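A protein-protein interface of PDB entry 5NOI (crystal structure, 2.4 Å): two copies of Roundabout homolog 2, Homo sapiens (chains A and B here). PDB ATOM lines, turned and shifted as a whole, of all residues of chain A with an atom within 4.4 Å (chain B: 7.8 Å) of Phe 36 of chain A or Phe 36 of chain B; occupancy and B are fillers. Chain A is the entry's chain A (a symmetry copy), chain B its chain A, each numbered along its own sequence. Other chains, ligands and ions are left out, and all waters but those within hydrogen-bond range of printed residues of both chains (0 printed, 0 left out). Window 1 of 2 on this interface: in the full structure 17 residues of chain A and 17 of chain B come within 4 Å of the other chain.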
ATOM      1  N   ALA A  34      -8.166  -1.263 -31.949  1.00  0.00           N
ATOM      2  CA  ALA A  34      -8.804  -0.807 -30.721  1.00  0.00           C
ATOM      3  C   ALA A  34      -8.337  -1.729 -29.588  1.00  0.00           C
ATOM      4  O   ALA A  34      -8.682  -2.915 -29.565  1.00  0.00           O
ATOM      5  CB  ALA A  34     -10.325  -0.810 -30.890  1.00  0.00           C
ATOM      6  N   VAL A  35      -7.522  -1.182 -28.666  1.00  0.00           N
ATOM      7  CA  VAL A  35      -6.933  -1.982 -27.600  1.00  0.00           C
ATOM      8  C   VAL A  35      -7.943  -2.201 -26.465  1.00  0.00           C
ATOM      9  O   VAL A  35      -8.674  -1.283 -26.066  1.00  0.00           O
ATOM     10  CB  VAL A  35      -5.645  -1.302 -27.089  1.00  0.00           C
ATOM     11  CG1 VAL A  35      -5.370  -1.660 -25.678  1.00  0.00           C
ATOM     12  CG2 VAL A  35      -4.440  -1.638 -27.964  1.00  0.00           C
ATOM     13  N   PHE A  36      -7.958  -3.418 -25.922  1.00  0.00           N
ATOM     14  CA  PHE A  36      -8.638  -3.699 -24.660  1.00  0.00           C
ATOM     15  C   PHE A  36      -7.678  -4.446 -23.743  1.00  0.00           C
ATOM     16  O   PHE A  36      -6.670  -4.998 -24.189  1.00  0.00           O
ATOM     17  CB  PHE A  36      -9.946  -4.499 -24.850  1.00  0.00           C
ATOM     18  CG  PHE A  36      -9.756  -5.890 -25.426  1.00  0.00           C
ATOM     19  CD1 PHE A  36      -9.821  -6.104 -26.797  1.00  0.00           C
ATOM     20  CD2 PHE A  36      -9.552  -6.988 -24.602  1.00  0.00           C
ATOM     21  CE1 PHE A  36      -9.654  -7.387 -27.332  1.00  0.00           C
ATOM     22  CE2 PHE A  36      -9.389  -8.252 -25.123  1.00  0.00           C
ATOM     23  CZ  PHE A  36      -9.456  -8.459 -26.489  1.00  0.00           C
ATOM     24  N   TRP A  37      -7.987  -4.447 -22.447  1.00  0.00           N
ATOM     25  CA  TRP A  37      -7.119  -5.061 -21.447  1.00  0.00           C
ATOM     26  C   TRP A  37      -7.848  -6.171 -20.696  1.00  0.00           C
ATOM     27  O   TRP A  37      -9.082  -6.210 -20.615  1.00  0.00           O
ATOM     28  CB  TRP A  37      -6.603  -4.035 -20.434  1.00  0.00           C
ATOM     29  CG  TRP A  37      -5.606  -3.042 -20.972  1.00  0.00           C
ATOM     30  CD1 TRP A  37      -5.870  -1.938 -21.743  1.00  0.00           C
ATOM     31  CD2 TRP A  37      -4.186  -3.034 -20.754  1.00  0.00           C
ATOM     32  NE1 TRP A  37      -4.716  -1.251 -22.012  1.00  0.00           N
ATOM     33  CE2 TRP A  37      -3.664  -1.909 -21.429  1.00  0.00           C
ATOM     34  CE3 TRP A  37      -3.304  -3.878 -20.066  1.00  0.00           C
ATOM     35  CZ2 TRP A  37      -2.303  -1.599 -21.418  1.00  0.00           C
ATOM     36  CZ3 TRP A  37      -1.943  -3.569 -20.066  1.00  0.00           C
ATOM     37  CH2 TRP A  37      -1.461  -2.443 -20.735  1.00  0.00           C
ATOM     38  N   LEU A  45     -13.072  -8.408 -19.290  1.00  0.00           N
ATOM     39  CA  LEU A  45     -12.377  -7.585 -20.249  1.00  0.00           C
ATOM     40  C   LEU A  45     -12.695  -6.118 -20.003  1.00  0.00           C
ATOM     41  O   LEU A  45     -13.813  -5.759 -19.625  1.00  0.00           O
ATOM     42  CB  LEU A  45     -12.731  -7.974 -21.677  1.00  0.00           C
ATOM     43  CG  LEU A  45     -12.627  -9.459 -21.957  1.00  0.00           C
ATOM     44  CD1 LEU A  45     -13.203  -9.857 -23.323  1.00  0.00           C
ATOM     45  CD2 LEU A  45     -11.172  -9.847 -21.810  1.00  0.00           C
ATOM     46  N   LEU A  46     -11.684  -5.276 -20.231  1.00  0.00           N
ATOM     47  CA  LEU A  46     -11.801  -3.832 -20.052  1.00  0.00           C
ATOM     48  C   LEU A  46     -11.721  -3.145 -21.414  1.00  0.00           C
ATOM     49  O   LEU A  46     -10.645  -3.028 -21.997  1.00  0.00           O
ATOM     50  CB  LEU A  46     -10.732  -3.337 -19.086  1.00  0.00           C
ATOM     51  CG  LEU A  46     -10.577  -4.226 -17.862  1.00  0.00           C
ATOM     52  CD1 LEU A  46      -9.432  -3.799 -16.924  1.00  0.00           C
ATOM     53  CD2 LEU A  46     -11.906  -4.209 -17.159  1.00  0.00           C
ATOM     54  N   PHE A  47     -12.817  -2.691 -21.888  1.00  0.00           N
ATOM     55  CA  PHE A  47     -13.063  -2.068 -23.182  1.00  0.00           C
ATOM     56  C   PHE A  47     -13.019  -0.540 -23.086  1.00  0.00           C
ATOM     57  O   PHE A  47     -13.346   0.041 -22.046  1.00  0.00           O
ATOM     58  CB  PHE A  47     -14.412  -2.516 -23.750  1.00  0.00           C
ATOM     59  CG  PHE A  47     -14.365  -3.856 -24.418  1.00  0.00           C
ATOM     60  CD1 PHE A  47     -15.302  -4.207 -25.395  1.00  0.00           C
ATOM     61  CD2 PHE A  47     -13.392  -4.775 -24.068  1.00  0.00           C
ATOM     62  CE1 PHE A  47     -15.227  -5.459 -26.023  1.00  0.00           C
ATOM     63  CE2 PHE A  47     -13.316  -6.010 -24.675  1.00  0.00           C
ATOM     64  CZ  PHE A  47     -14.210  -6.361 -25.630  1.00  0.00           C
ATOM     65  N   ILE A  80      -2.818  -7.898 -19.559  1.00  0.00           N
ATOM     66  CA  ILE A  80      -2.626  -8.184 -20.974  1.00  0.00           C
ATOM     67  C   ILE A  80      -3.317  -7.102 -21.800  1.00  0.00           C
ATOM     68  O   ILE A  80      -4.532  -6.921 -21.693  1.00  0.00           O
ATOM     69  CB  ILE A  80      -3.197  -9.562 -21.333  1.00  0.00           C
ATOM     70  CG1 ILE A  80      -2.646 -10.644 -20.401  1.00  0.00           C
ATOM     71  CG2 ILE A  80      -2.940  -9.901 -22.830  1.00  0.00           C
ATOM     72  CD1 ILE A  80      -3.336 -11.958 -20.604  1.00  0.00           C
ATOM     73  N   CYS A  81      -2.573  -6.401 -22.660  1.00  0.00           N
ATOM     74  CA  CYS A  81      -3.213  -5.490 -23.601  1.00  0.00           C
ATOM     75  C   CYS A  81      -3.264  -6.153 -24.964  1.00  0.00           C
ATOM     76  O   CYS A  81      -2.322  -6.840 -25.373  1.00  0.00           O
ATOM     77  CB  CYS A  81      -2.533  -4.125 -23.665  1.00  0.00           C
ATOM     78  SG  CYS A  81      -1.111  -3.888 -24.727  1.00  0.00           S
ATOM     79  N   GLN A  82      -4.402  -5.994 -25.627  1.00  0.00           N
ATOM     80  CA  GLN A  82      -4.803  -6.856 -26.722  1.00  0.00           C
ATOM     81  C   GLN A  82      -5.505  -6.034 -27.793  1.00  0.00           C
ATOM     82  O   GLN A  82      -6.079  -4.973 -27.525  1.00  0.00           O
ATOM     83  CB  GLN A  82      -5.735  -7.951 -26.232  1.00  0.00           C
ATOM     84  CG  GLN A  82      -5.014  -9.048 -25.525  1.00  0.00           C
ATOM     85  CD  GLN A  82      -5.939  -9.957 -24.801  1.00  0.00           C
ATOM     86  OE1 GLN A  82      -6.273 -11.021 -25.310  1.00  0.00           O
ATOM     87  NE2 GLN A  82      -6.377  -9.546 -23.600  1.00  0.00           N
ATOM     88  N   LEU A  84      -7.569  -6.801 -31.784  1.00  0.00           N
ATOM     89  CA  LEU A  84      -7.985  -7.704 -32.851  1.00  0.00           C
ATOM     90  C   LEU A  84      -8.615  -6.886 -33.980  1.00  0.00           C
ATOM     91  O   LEU A  84      -9.494  -6.051 -33.732  1.00  0.00           O
ATOM     92  CB  LEU A  84      -8.941  -8.764 -32.299  1.00  0.00           C
ATOM     93  CG  LEU A  84      -9.651  -9.721 -33.199  1.00  0.00           C
ATOM     94  CD1 LEU A  84      -8.744 -10.397 -34.125  1.00  0.00           C
ATOM     95  CD2 LEU A  84     -10.407 -10.745 -32.409  1.00  0.00           C
ATOM     96  N   CYS B  25     -21.817 -15.984 -35.592  1.00  0.00           N
ATOM     97  CA  CYS B  25     -21.815 -14.643 -35.022  1.00  0.00           C
ATOM     98  C   CYS B  25     -21.349 -13.731 -36.148  1.00  0.00           C
ATOM     99  O   CYS B  25     -20.145 -13.474 -36.295  1.00  0.00           O
ATOM    100  CB  CYS B  25     -20.928 -14.559 -33.785  1.00  0.00           C
ATOM    101  SG  CYS B  25     -20.787 -12.940 -33.004  1.00  0.00           S
ATOM    102  N   PRO B  33     -15.852  -5.584 -38.195  1.00  0.00           N
ATOM    103  CA  PRO B  33     -15.525  -6.131 -36.870  1.00  0.00           C
ATOM    104  C   PRO B  33     -14.964  -7.536 -36.976  1.00  0.00           C
ATOM    105  O   PRO B  33     -15.450  -8.372 -37.744  1.00  0.00           O
ATOM    106  CB  PRO B  33     -16.868  -6.112 -36.136  1.00  0.00           C
ATOM    107  CG  PRO B  33     -17.683  -5.046 -36.894  1.00  0.00           C
ATOM    108  CD  PRO B  33     -17.274  -5.210 -38.308  1.00  0.00           C
ATOM    109  N   ALA B  34     -13.898  -7.774 -36.214  1.00  0.00           N
ATOM    110  CA  ALA B  34     -13.286  -9.091 -36.094  1.00  0.00           C
ATOM    111  C   ALA B  34     -13.800  -9.722 -34.793  1.00  0.00           C
ATOM    112  O   ALA B  34     -13.477  -9.249 -33.698  1.00  0.00           O
ATOM    113  CB  ALA B  34     -11.762  -8.964 -36.121  1.00  0.00           C
ATOM    114  N   VAL B  35     -14.629 -10.775 -34.923  1.00  0.00           N
ATOM    115  CA  VAL B  35     -15.262 -11.393 -33.765  1.00  0.00           C
ATOM    116  C   VAL B  35     -14.288 -12.348 -33.062  1.00  0.00           C
ATOM    117  O   VAL B  35     -13.552 -13.109 -33.705  1.00  0.00           O
ATOM    118  CB  VAL B  35     -16.551 -12.121 -34.202  1.00  0.00           C
ATOM    119  CG1 VAL B  35     -16.871 -13.244 -33.291  1.00  0.00           C
ATOM    120  CG2 VAL B  35     -17.738 -11.165 -34.298  1.00  0.00           C
ATOM    121  N   PHE B  36     -14.309 -12.327 -31.729  1.00  0.00           N
ATOM    122  CA  PHE B  36     -13.668 -13.365 -30.924  1.00  0.00           C
ATOM    123  C   PHE B  36     -14.665 -13.864 -29.887  1.00  0.00           C
ATOM    124  O   PHE B  36     -15.670 -13.210 -29.602  1.00  0.00           O
ATOM    125  CB  PHE B  36     -12.370 -12.878 -30.243  1.00  0.00           C
ATOM    126  CG  PHE B  36     -12.566 -11.767 -29.229  1.00  0.00           C
ATOM    127  CD1 PHE B  36     -12.469 -10.434 -29.611  1.00  0.00           C
ATOM    128  CD2 PHE B  36     -12.813 -12.047 -27.893  1.00  0.00           C
ATOM    129  CE1 PHE B  36     -12.643  -9.406 -28.677  1.00  0.00           C
ATOM    130  CE2 PHE B  36     -12.984 -11.040 -26.970  1.00  0.00           C
ATOM    131  CZ  PHE B  36     -12.883  -9.715 -27.356  1.00  0.00           C
ATOM    132  N   TRP B  37     -14.392 -15.045 -29.332  1.00  0.00           N
ATOM    133  CA  TRP B  37     -15.297 -15.677 -28.378  1.00  0.00           C
ATOM    134  C   TRP B  37     -14.609 -15.903 -27.036  1.00  0.00           C
ATOM    135  O   TRP B  37     -13.377 -15.982 -26.933  1.00  0.00           O
ATOM    136  CB  TRP B  37     -15.823 -17.020 -28.896  1.00  0.00           C
ATOM    137  CG  TRP B  37     -16.787 -16.933 -30.050  1.00  0.00           C
ATOM    138  CD1 TRP B  37     -16.482 -16.704 -31.369  1.00  0.00           C
ATOM    139  CD2 TRP B  37     -18.212 -17.109 -30.004  1.00  0.00           C
ATOM    140  NE1 TRP B  37     -17.618 -16.730 -32.136  1.00  0.00           N
ATOM    141  CE2 TRP B  37     -18.695 -16.962 -31.323  1.00  0.00           C
ATOM    142  CE3 TRP B  37     -19.127 -17.362 -28.974  1.00  0.00           C
ATOM    143  CZ2 TRP B  37     -20.052 -17.079 -31.636  1.00  0.00           C
ATOM    144  CZ3 TRP B  37     -20.482 -17.469 -29.291  1.00  0.00           C
ATOM    145  CH2 TRP B  37     -20.925 -17.329 -30.607  1.00  0.00           C
ATOM    146  N   GLN B  38     -15.442 -16.051 -26.014  1.00  0.00           N
ATOM    147  CA  GLN B  38     -14.979 -16.282 -24.655  1.00  0.00           C
ATOM    148  C   GLN B  38     -16.052 -17.090 -23.961  1.00  0.00           C
ATOM    149  O   GLN B  38     -17.210 -16.660 -23.930  1.00  0.00           O
ATOM    150  CB  GLN B  38     -14.753 -14.959 -23.931  1.00  0.00           C
ATOM    151  CG  GLN B  38     -14.444 -15.081 -22.474  1.00  0.00           C
ATOM    152  CD  GLN B  38     -14.403 -13.734 -21.795  1.00  0.00           C
ATOM    153  OE1 GLN B  38     -14.872 -12.730 -22.336  1.00  0.00           O
ATOM    154  NE2 GLN B  38     -13.823 -13.697 -20.607  1.00  0.00           N
ATOM    155  N   ASN B  44      -9.804 -17.571 -21.035  1.00  0.00           N
ATOM    156  CA  ASN B  44      -9.299 -17.813 -22.377  1.00  0.00           C
ATOM    157  C   ASN B  44     -10.135 -17.068 -23.406  1.00  0.00           C
ATOM    158  O   ASN B  44     -11.367 -17.168 -23.411  1.00  0.00           O
ATOM    159  CB  ASN B  44      -9.304 -19.303 -22.685  1.00  0.00           C
ATOM    160  CG  ASN B  44      -8.635 -20.098 -21.606  1.00  0.00           C
ATOM    161  OD1 ASN B  44      -9.227 -21.018 -21.030  1.00  0.00           O
ATOM    162  ND2 ASN B  44      -7.391 -19.734 -21.298  1.00  0.00           N
ATOM    163  N   LEU B  45      -9.464 -16.327 -24.273  1.00  0.00           N
ATOM    164  CA  LEU B  45     -10.119 -15.792 -25.443  1.00  0.00           C
ATOM    165  C   LEU B  45      -9.783 -16.639 -26.660  1.00  0.00           C
ATOM    166  O   LEU B  45      -8.669 -17.152 -26.795  1.00  0.00           O
ATOM    167  CB  LEU B  45      -9.732 -14.339 -25.681  1.00  0.00           C
ATOM    168  CG  LEU B  45      -9.854 -13.458 -24.455  1.00  0.00           C
ATOM    169  CD1 LEU B  45      -9.250 -12.061 -24.653  1.00  0.00           C
ATOM    170  CD2 LEU B  45     -11.320 -13.402 -24.081  1.00  0.00           C
ATOM    171  N   LEU B  46     -10.772 -16.769 -27.547  1.00  0.00           N
ATOM    172  CA  LEU B  46     -10.635 -17.542 -28.777  1.00  0.00           C
ATOM    173  C   LEU B  46     -10.665 -16.596 -29.976  1.00  0.00           C
ATOM    174  O   LEU B  46     -11.723 -16.097 -30.357  1.00  0.00           O
ATOM    175  CB  LEU B  46     -11.720 -18.608 -28.849  1.00  0.00           C
ATOM    176  CG  LEU B  46     -11.924 -19.341 -27.532  1.00  0.00           C
ATOM    177  CD1 LEU B  46     -13.087 -20.351 -27.556  1.00  0.00           C
ATOM    178  CD2 LEU B  46     -10.614 -20.008 -27.215  1.00  0.00           C
ATOM    179  N   PHE B  47      -9.548 -16.376 -30.557  1.00  0.00           N
ATOM    180  CA  PHE B  47      -9.257 -15.470 -31.661  1.00  0.00           C
ATOM    181  C   PHE B  47      -9.277 -16.200 -33.006  1.00  0.00           C
ATOM    182  O   PHE B  47      -8.969 -17.394 -33.087  1.00  0.00           O
ATOM    183  CB  PHE B  47      -7.900 -14.789 -31.456  1.00  0.00           C
ATOM    184  CG  PHE B  47      -7.953 -13.618 -30.524  1.00  0.00           C
ATOM    185  CD1 PHE B  47      -6.997 -12.600 -30.592  1.00  0.00           C
ATOM    186  CD2 PHE B  47      -8.952 -13.531 -29.570  1.00  0.00           C
ATOM    187  CE1 PHE B  47      -7.076 -11.502 -29.723  1.00  0.00           C
ATOM    188  CE2 PHE B  47      -9.031 -12.459 -28.708  1.00  0.00           C
ATOM    189  CZ  PHE B  47      -8.119 -11.460 -28.767  1.00  0.00           C
ATOM    190  N   PRO B  48      -9.680 -15.494 -34.063  1.00  0.00           N
ATOM    191  CA  PRO B  48      -9.899 -16.156 -35.361  1.00  0.00           C
ATOM    192  C   PRO B  48      -8.681 -16.811 -36.012  1.00  0.00           C
ATOM    193  O   PRO B  48      -8.813 -17.945 -36.488  1.00  0.00           O
ATOM    194  CB  PRO B  48     -10.459 -15.014 -36.228  1.00  0.00           C
ATOM    195  CG  PRO B  48     -10.147 -13.750 -35.486  1.00  0.00           C
ATOM    196  CD  PRO B  48     -10.267 -14.151 -34.046  1.00  0.00           C
ATOM    197  N   VAL B  60     -12.368 -20.592 -33.862  1.00  0.00           N
ATOM    198  CA  VAL B  60     -13.137 -19.457 -34.333  1.00  0.00           C
ATOM    199  C   VAL B  60     -12.692 -19.172 -35.764  1.00  0.00           C
ATOM    200  O   VAL B  60     -11.487 -19.126 -36.048  1.00  0.00           O
ATOM    201  CB  VAL B  60     -12.933 -18.250 -33.403  1.00  0.00           C
ATOM    202  CG1 VAL B  60     -13.352 -17.015 -34.024  1.00  0.00           C
ATOM    203  CG2 VAL B  60     -13.650 -18.461 -32.118  1.00  0.00           C
ATOM    204  N   SER B  61     -13.653 -19.058 -36.691  1.00  0.00           N
ATOM    205  CA  SER B  61     -13.296 -18.800 -38.070  1.00  0.00           C
ATOM    206  C   SER B  61     -13.271 -17.304 -38.303  1.00  0.00           C
ATOM    207  O   SER B  61     -13.712 -16.530 -37.447  1.00  0.00           O
ATOM    208  CB  SER B  61     -14.283 -19.487 -39.016  1.00  0.00           C
ATOM    209  OG  SER B  61     -15.619 -19.110 -38.747  1.00  0.00           O
ATOM    210  N   GLY B  64     -16.580 -15.528 -37.980  1.00  0.00           N
ATOM    211  CA  GLY B  64     -17.131 -15.322 -36.665  1.00  0.00           C
ATOM    212  C   GLY B  64     -17.733 -16.562 -36.045  1.00  0.00           C
ATOM    213  O   GLY B  64     -18.307 -16.467 -34.956  1.00  0.00           O
ATOM    214  N   LEU B  66     -17.924 -20.027 -34.052  1.00  0.00           N
ATOM    215  CA  LEU B  66     -17.253 -20.764 -32.994  1.00  0.00           C
ATOM    216  C   LEU B  66     -17.622 -22.222 -33.194  1.00  0.00           C
ATOM    217  O   LEU B  66     -18.789 -22.599 -33.040  1.00  0.00           O
ATOM    218  CB  LEU B  66     -17.673 -20.268 -31.614  1.00  0.00           C
ATOM    219  CG  LEU B  66     -17.397 -21.150 -30.500  1.00  0.00           C
ATOM    220  CD1 LEU B  66     -16.004 -21.427 -30.344  1.00  0.00           C
ATOM    221  CD2 LEU B  66     -17.939 -20.624 -29.207  1.00  0.00           C
ATOM    222  N   TYR B  79     -21.465 -18.819 -23.892  1.00  0.00           N
ATOM    223  CA  TYR B  79     -20.362 -18.426 -24.772  1.00  0.00           C
ATOM    224  C   TYR B  79     -20.632 -17.035 -25.337  1.00  0.00           C
ATOM    225  O   TYR B  79     -21.672 -16.809 -25.965  1.00  0.00           O
ATOM    226  CB  TYR B  79     -20.198 -19.436 -25.908  1.00  0.00           C
ATOM    227  CG  TYR B  79     -19.652 -20.753 -25.433  1.00  0.00           C
ATOM    228  CD1 TYR B  79     -18.294 -20.930 -25.262  1.00  0.00           C
ATOM    229  CD2 TYR B  79     -20.496 -21.815 -25.129  1.00  0.00           C
ATOM    230  CE1 TYR B  79     -17.780 -22.116 -24.832  1.00  0.00           C
ATOM    231  CE2 TYR B  79     -19.981 -23.009 -24.681  1.00  0.00           C
ATOM    232  CZ  TYR B  79     -18.628 -23.150 -24.540  1.00  0.00           C
ATOM    233  OH  TYR B  79     -18.104 -24.328 -24.106  1.00  0.00           O
ATOM    234  N   ILE B  80     -19.697 -16.119 -25.128  1.00  0.00           N
ATOM    235  CA  ILE B  80     -19.855 -14.712 -25.470  1.00  0.00           C
ATOM    236  C   ILE B  80     -19.124 -14.431 -26.780  1.00  0.00           C
ATOM    237  O   ILE B  80     -17.909 -14.625 -26.866  1.00  0.00           O
ATOM    238  CB  ILE B  80     -19.299 -13.816 -24.356  1.00  0.00           C
ATOM    239  CG1 ILE B  80     -19.894 -14.195 -22.998  1.00  0.00           C
ATOM    240  CG2 ILE B  80     -19.520 -12.312 -24.686  1.00  0.00           C
ATOM    241  CD1 ILE B  80     -19.222 -13.469 -21.873  1.00  0.00           C
ATOM    242  N   CYS B  81     -19.832 -13.934 -27.798  1.00  0.00           N
ATOM    243  CA  CYS B  81     -19.151 -13.476 -29.003  1.00  0.00           C
ATOM    244  C   CYS B  81     -19.073 -11.962 -28.974  1.00  0.00           C
ATOM    245  O   CYS B  81     -20.016 -11.285 -28.549  1.00  0.00           O
ATOM    246  CB  CYS B  81     -19.804 -13.981 -30.286  1.00  0.00           C
ATOM    247  SG  CYS B  81     -21.193 -13.093 -30.987  1.00  0.00           S
ATOM    248  N   GLN B  82     -17.915 -11.448 -29.366  1.00  0.00           N
ATOM    249  CA  GLN B  82     -17.499 -10.099 -29.035  1.00  0.00           C
ATOM    250  C   GLN B  82     -16.754  -9.486 -30.212  1.00  0.00           C
ATOM    251  O   GLN B  82     -16.169 -10.186 -31.045  1.00  0.00           O
ATOM    252  CB  GLN B  82     -16.601 -10.097 -27.810  1.00  0.00           C
ATOM    253  CG  GLN B  82     -17.360 -10.263 -26.538  1.00  0.00           C
ATOM    254  CD  GLN B  82     -16.470 -10.552 -25.383  1.00  0.00           C
ATOM    255  OE1 GLN B  82     -16.140  -9.649 -24.624  1.00  0.00           O
ATOM    256  NE2 GLN B  82     -16.058 -11.823 -25.238  1.00  0.00           N
ATOM    257  N   ALA B  83     -16.770  -8.163 -30.270  1.00  0.00           N
ATOM    258  CA  ALA B  83     -16.093  -7.466 -31.353  1.00  0.00           C
ATOM    259  C   ALA B  83     -15.816  -6.056 -30.895  1.00  0.00           C
ATOM    260  O   ALA B  83     -16.710  -5.411 -30.336  1.00  0.00           O
ATOM    261  CB  ALA B  83     -16.933  -7.452 -32.620  1.00  0.00           C
ATOM    262  N   LEU B  84     -14.595  -5.580 -31.140  1.00  0.00           N
ATOM    263  CA  LEU B  84     -14.167  -4.239 -30.759  1.00  0.00           C
ATOM    264  C   LEU B  84     -13.492  -3.572 -31.959  1.00  0.00           C
ATOM    265  O   LEU B  84     -12.606  -4.164 -32.587  1.00  0.00           O
ATOM    266  CB  LEU B  84     -13.244  -4.309 -29.539  1.00  0.00           C
ATOM    267  CG  LEU B  84     -12.528  -3.102 -29.031  1.00  0.00           C
ATOM    268  CD1 LEU B  84     -13.421  -1.962 -28.833  1.00  0.00           C
ATOM    269  CD2 LEU B  84     -11.811  -3.400 -27.749  1.00  0.00           C
ATOM    270  N   ILE B  90     -19.772  -4.715 -29.390  1.00  0.00           N
ATOM    271  CA  ILE B  90     -21.010  -5.489 -29.275  1.00  0.00           C
ATOM    272  C   ILE B  90     -20.689  -6.852 -28.675  1.00  0.00           C
ATOM    273  O   ILE B  90     -19.703  -7.489 -29.051  1.00  0.00           O
ATOM    274  CB  ILE B  90     -21.714  -5.688 -30.630  1.00  0.00           C
ATOM    275  CG1 ILE B  90     -20.767  -6.351 -31.619  1.00  0.00           C
ATOM    276  CG2 ILE B  90     -22.267  -4.374 -31.183  1.00  0.00           C
ATOM    277  CD1 ILE B  90     -21.291  -6.305 -33.053  1.00  0.00           C
ATOM    278  N   LEU B  91     -21.538  -7.314 -27.762  1.00  0.00           N
ATOM    279  CA  LEU B  91     -21.459  -8.707 -27.349  1.00  0.00           C
ATOM    280  C   LEU B  91     -22.832  -9.351 -27.490  1.00  0.00           C
ATOM    281  O   LEU B  91     -23.863  -8.681 -27.491  1.00  0.00           O
ATOM    282  CB  LEU B  91     -20.913  -8.845 -25.915  1.00  0.00           C
ATOM    283  CG  LEU B  91     -21.700  -8.225 -24.770  1.00  0.00           C
ATOM    284  CD1 LEU B  91     -22.535  -9.290 -24.063  1.00  0.00           C
ATOM    285  CD2 LEU B  91     -20.815  -7.485 -23.794  1.00  0.00           C
ATOM    286  N   ALA B  92     -22.802 -10.674 -27.610  1.00  0.00           N
ATOM    287  CA  ALA B  92     -23.992 -11.511 -27.667  1.00  0.00           C
ATOM    288  C   ALA B  92     -23.649 -12.847 -27.014  1.00  0.00           C
ATOM    289  O   ALA B  92     -22.603 -13.430 -27.319  1.00  0.00           O
ATOM    290  CB  ALA B  92     -24.452 -11.726 -29.108  1.00  0.00           C
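Among the printed residues, pairs that only touch across the chains: Leu 45 of chain A with Gln 82 of chain B (3.2 Å), Gln 82 of chain A with Leu 45 of chain B (3.2 Å), Leu 45 of chain A with Gln 38 of chain B (3.5 Å), Leu 84 of chain A with Phe 36 of chain B (3.5 Å), Phe 36 of chain A with Leu 84 of chain B (3.5 Å), Ala 34 of chain A with Leu 84 of chain B (3.7 Å), Leu 84 of chain A with Ala 34 of chain B (3.7 Å), Phe 36 of chain A with Phe 36 of chain B (3.8 Å), Leu 84 of chain A with Pro 48 of chain B (3.8 Å), Leu 84 of chain A with Leu 84 of chain B (3.8 Å), Leu 45 of chain A with Phe 36 of chain B (3.8 Å), Phe 36 of chain A with Leu 45 of chain B (3.8 Å), Phe 47 of chain A with Gln 82 of chain B (3.9 Å), Gln 82 of chain A with Phe 47 of chain B (3.9 Å), Phe 36 of chain A with Phe 47 of chain B (3.998 Å) and Phe 47 of chain A with Phe 36 of chain B (3.999 Å).
The backbone NH of Gln 82 of chain B lies within hydrogen-bond range of the backbone carbonyl oxygen of Phe 36 of chain B. The backbone carbonyl oxygen of Gln 38 of chain B lies within hydrogen-bond range of the backbone NH of Ile 80 of chain B (2.8 Å). The side-chain amide oxygen of Gln 38 of chain B is in hydrogen-bond range of the side-chain amide nitrogen of Gln 82 of chain B (3.3 Å). The backbone carbonyl oxygen (O) of Phe 36 of chain A sits at hydrogen-bond distance from the backbone NH (N) of Gln 82 of chain A (2.9 Å). The side-chain sulfur of Cys 25 of chain B forms a disulfide with the side-chain sulfur of Cys 81 of chain B, at 2.1 Å.
Ala 34 of chain A touches Leu 84 of chain B, and with the chains exchanged Leu 84 of chain A touches Ala 34 of chain B. Phe 36 of chain A touches Phe 47 of chain B, and with the chains exchanged Phe 47 of chain A touches Phe 36 of chain B. Phe 36 of chain A touches Leu 84 of chain B, and with the chains exchanged Leu 84 of chain A touches Phe 36 of chain B. Phe 47 of chain A touches Gln 82 of chain B, and with the chains exchanged Gln 82 of chain A touches Phe 47 of chain B. Positions printed for both chains: 34, 35, 36, 37, 45, 46, 47, 80, 81, 82 and 84. Of the 16 pairs that touch across the chains among the printed residues, 14 have their exchanged pair printed and touching as well.
Of the 25 printed residues of chain B, 8 touch a printed residue of chain A. Hydrophobic or aromatic side chains of chain B within 4 Å of the printed part of chain A: Ala 34, Phe 36, Leu 45, Phe 47, Pro 48 and Leu 84. Of the 11 printed residues of chain A, 6 touch a printed residue of chain B. Hydrophobic or aromatic side chains of chain A within 4 Å of the printed part of chain B: Ala 34, Phe 36, Leu 45, Phe 47 and Leu 84.
Printed residues of chain B within 4 Å of Phe 36 of chain A: Phe 36, Leu 45, Phe 47 and Leu 84. Printed residues of chain A within 4 Å of Phe 36 of chain B: Phe 36, Leu 45, Phe 47 and Leu 84. Of the printed residues of chain B, Ala 34 of chain A touches Leu 84 (3.7 Å). Of the printed residues of chain B, Leu 45 of chain A touches Phe 36, Gln 38 and Gln 82. Printed residues of chain B within 4 Å of Gln 82 of chain A: Leu 45 (3.2 Å) and Phe 47 (3.9 Å). Of the printed residues of chain B, Leu 84 of chain A touches Ala 34 (3.7 Å), Phe 36 (3.5 Å), Pro 48 (3.8 Å) and Leu 84 (3.8 Å). The nearest printed residue of chain B that does not touch Phe 36 of chain A is Gln 82 of chain B (6.9 Å). The nearest printed residue of chain B that does not touch Gln 82 of chain A is Leu 84 of chain B (5.9 Å).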
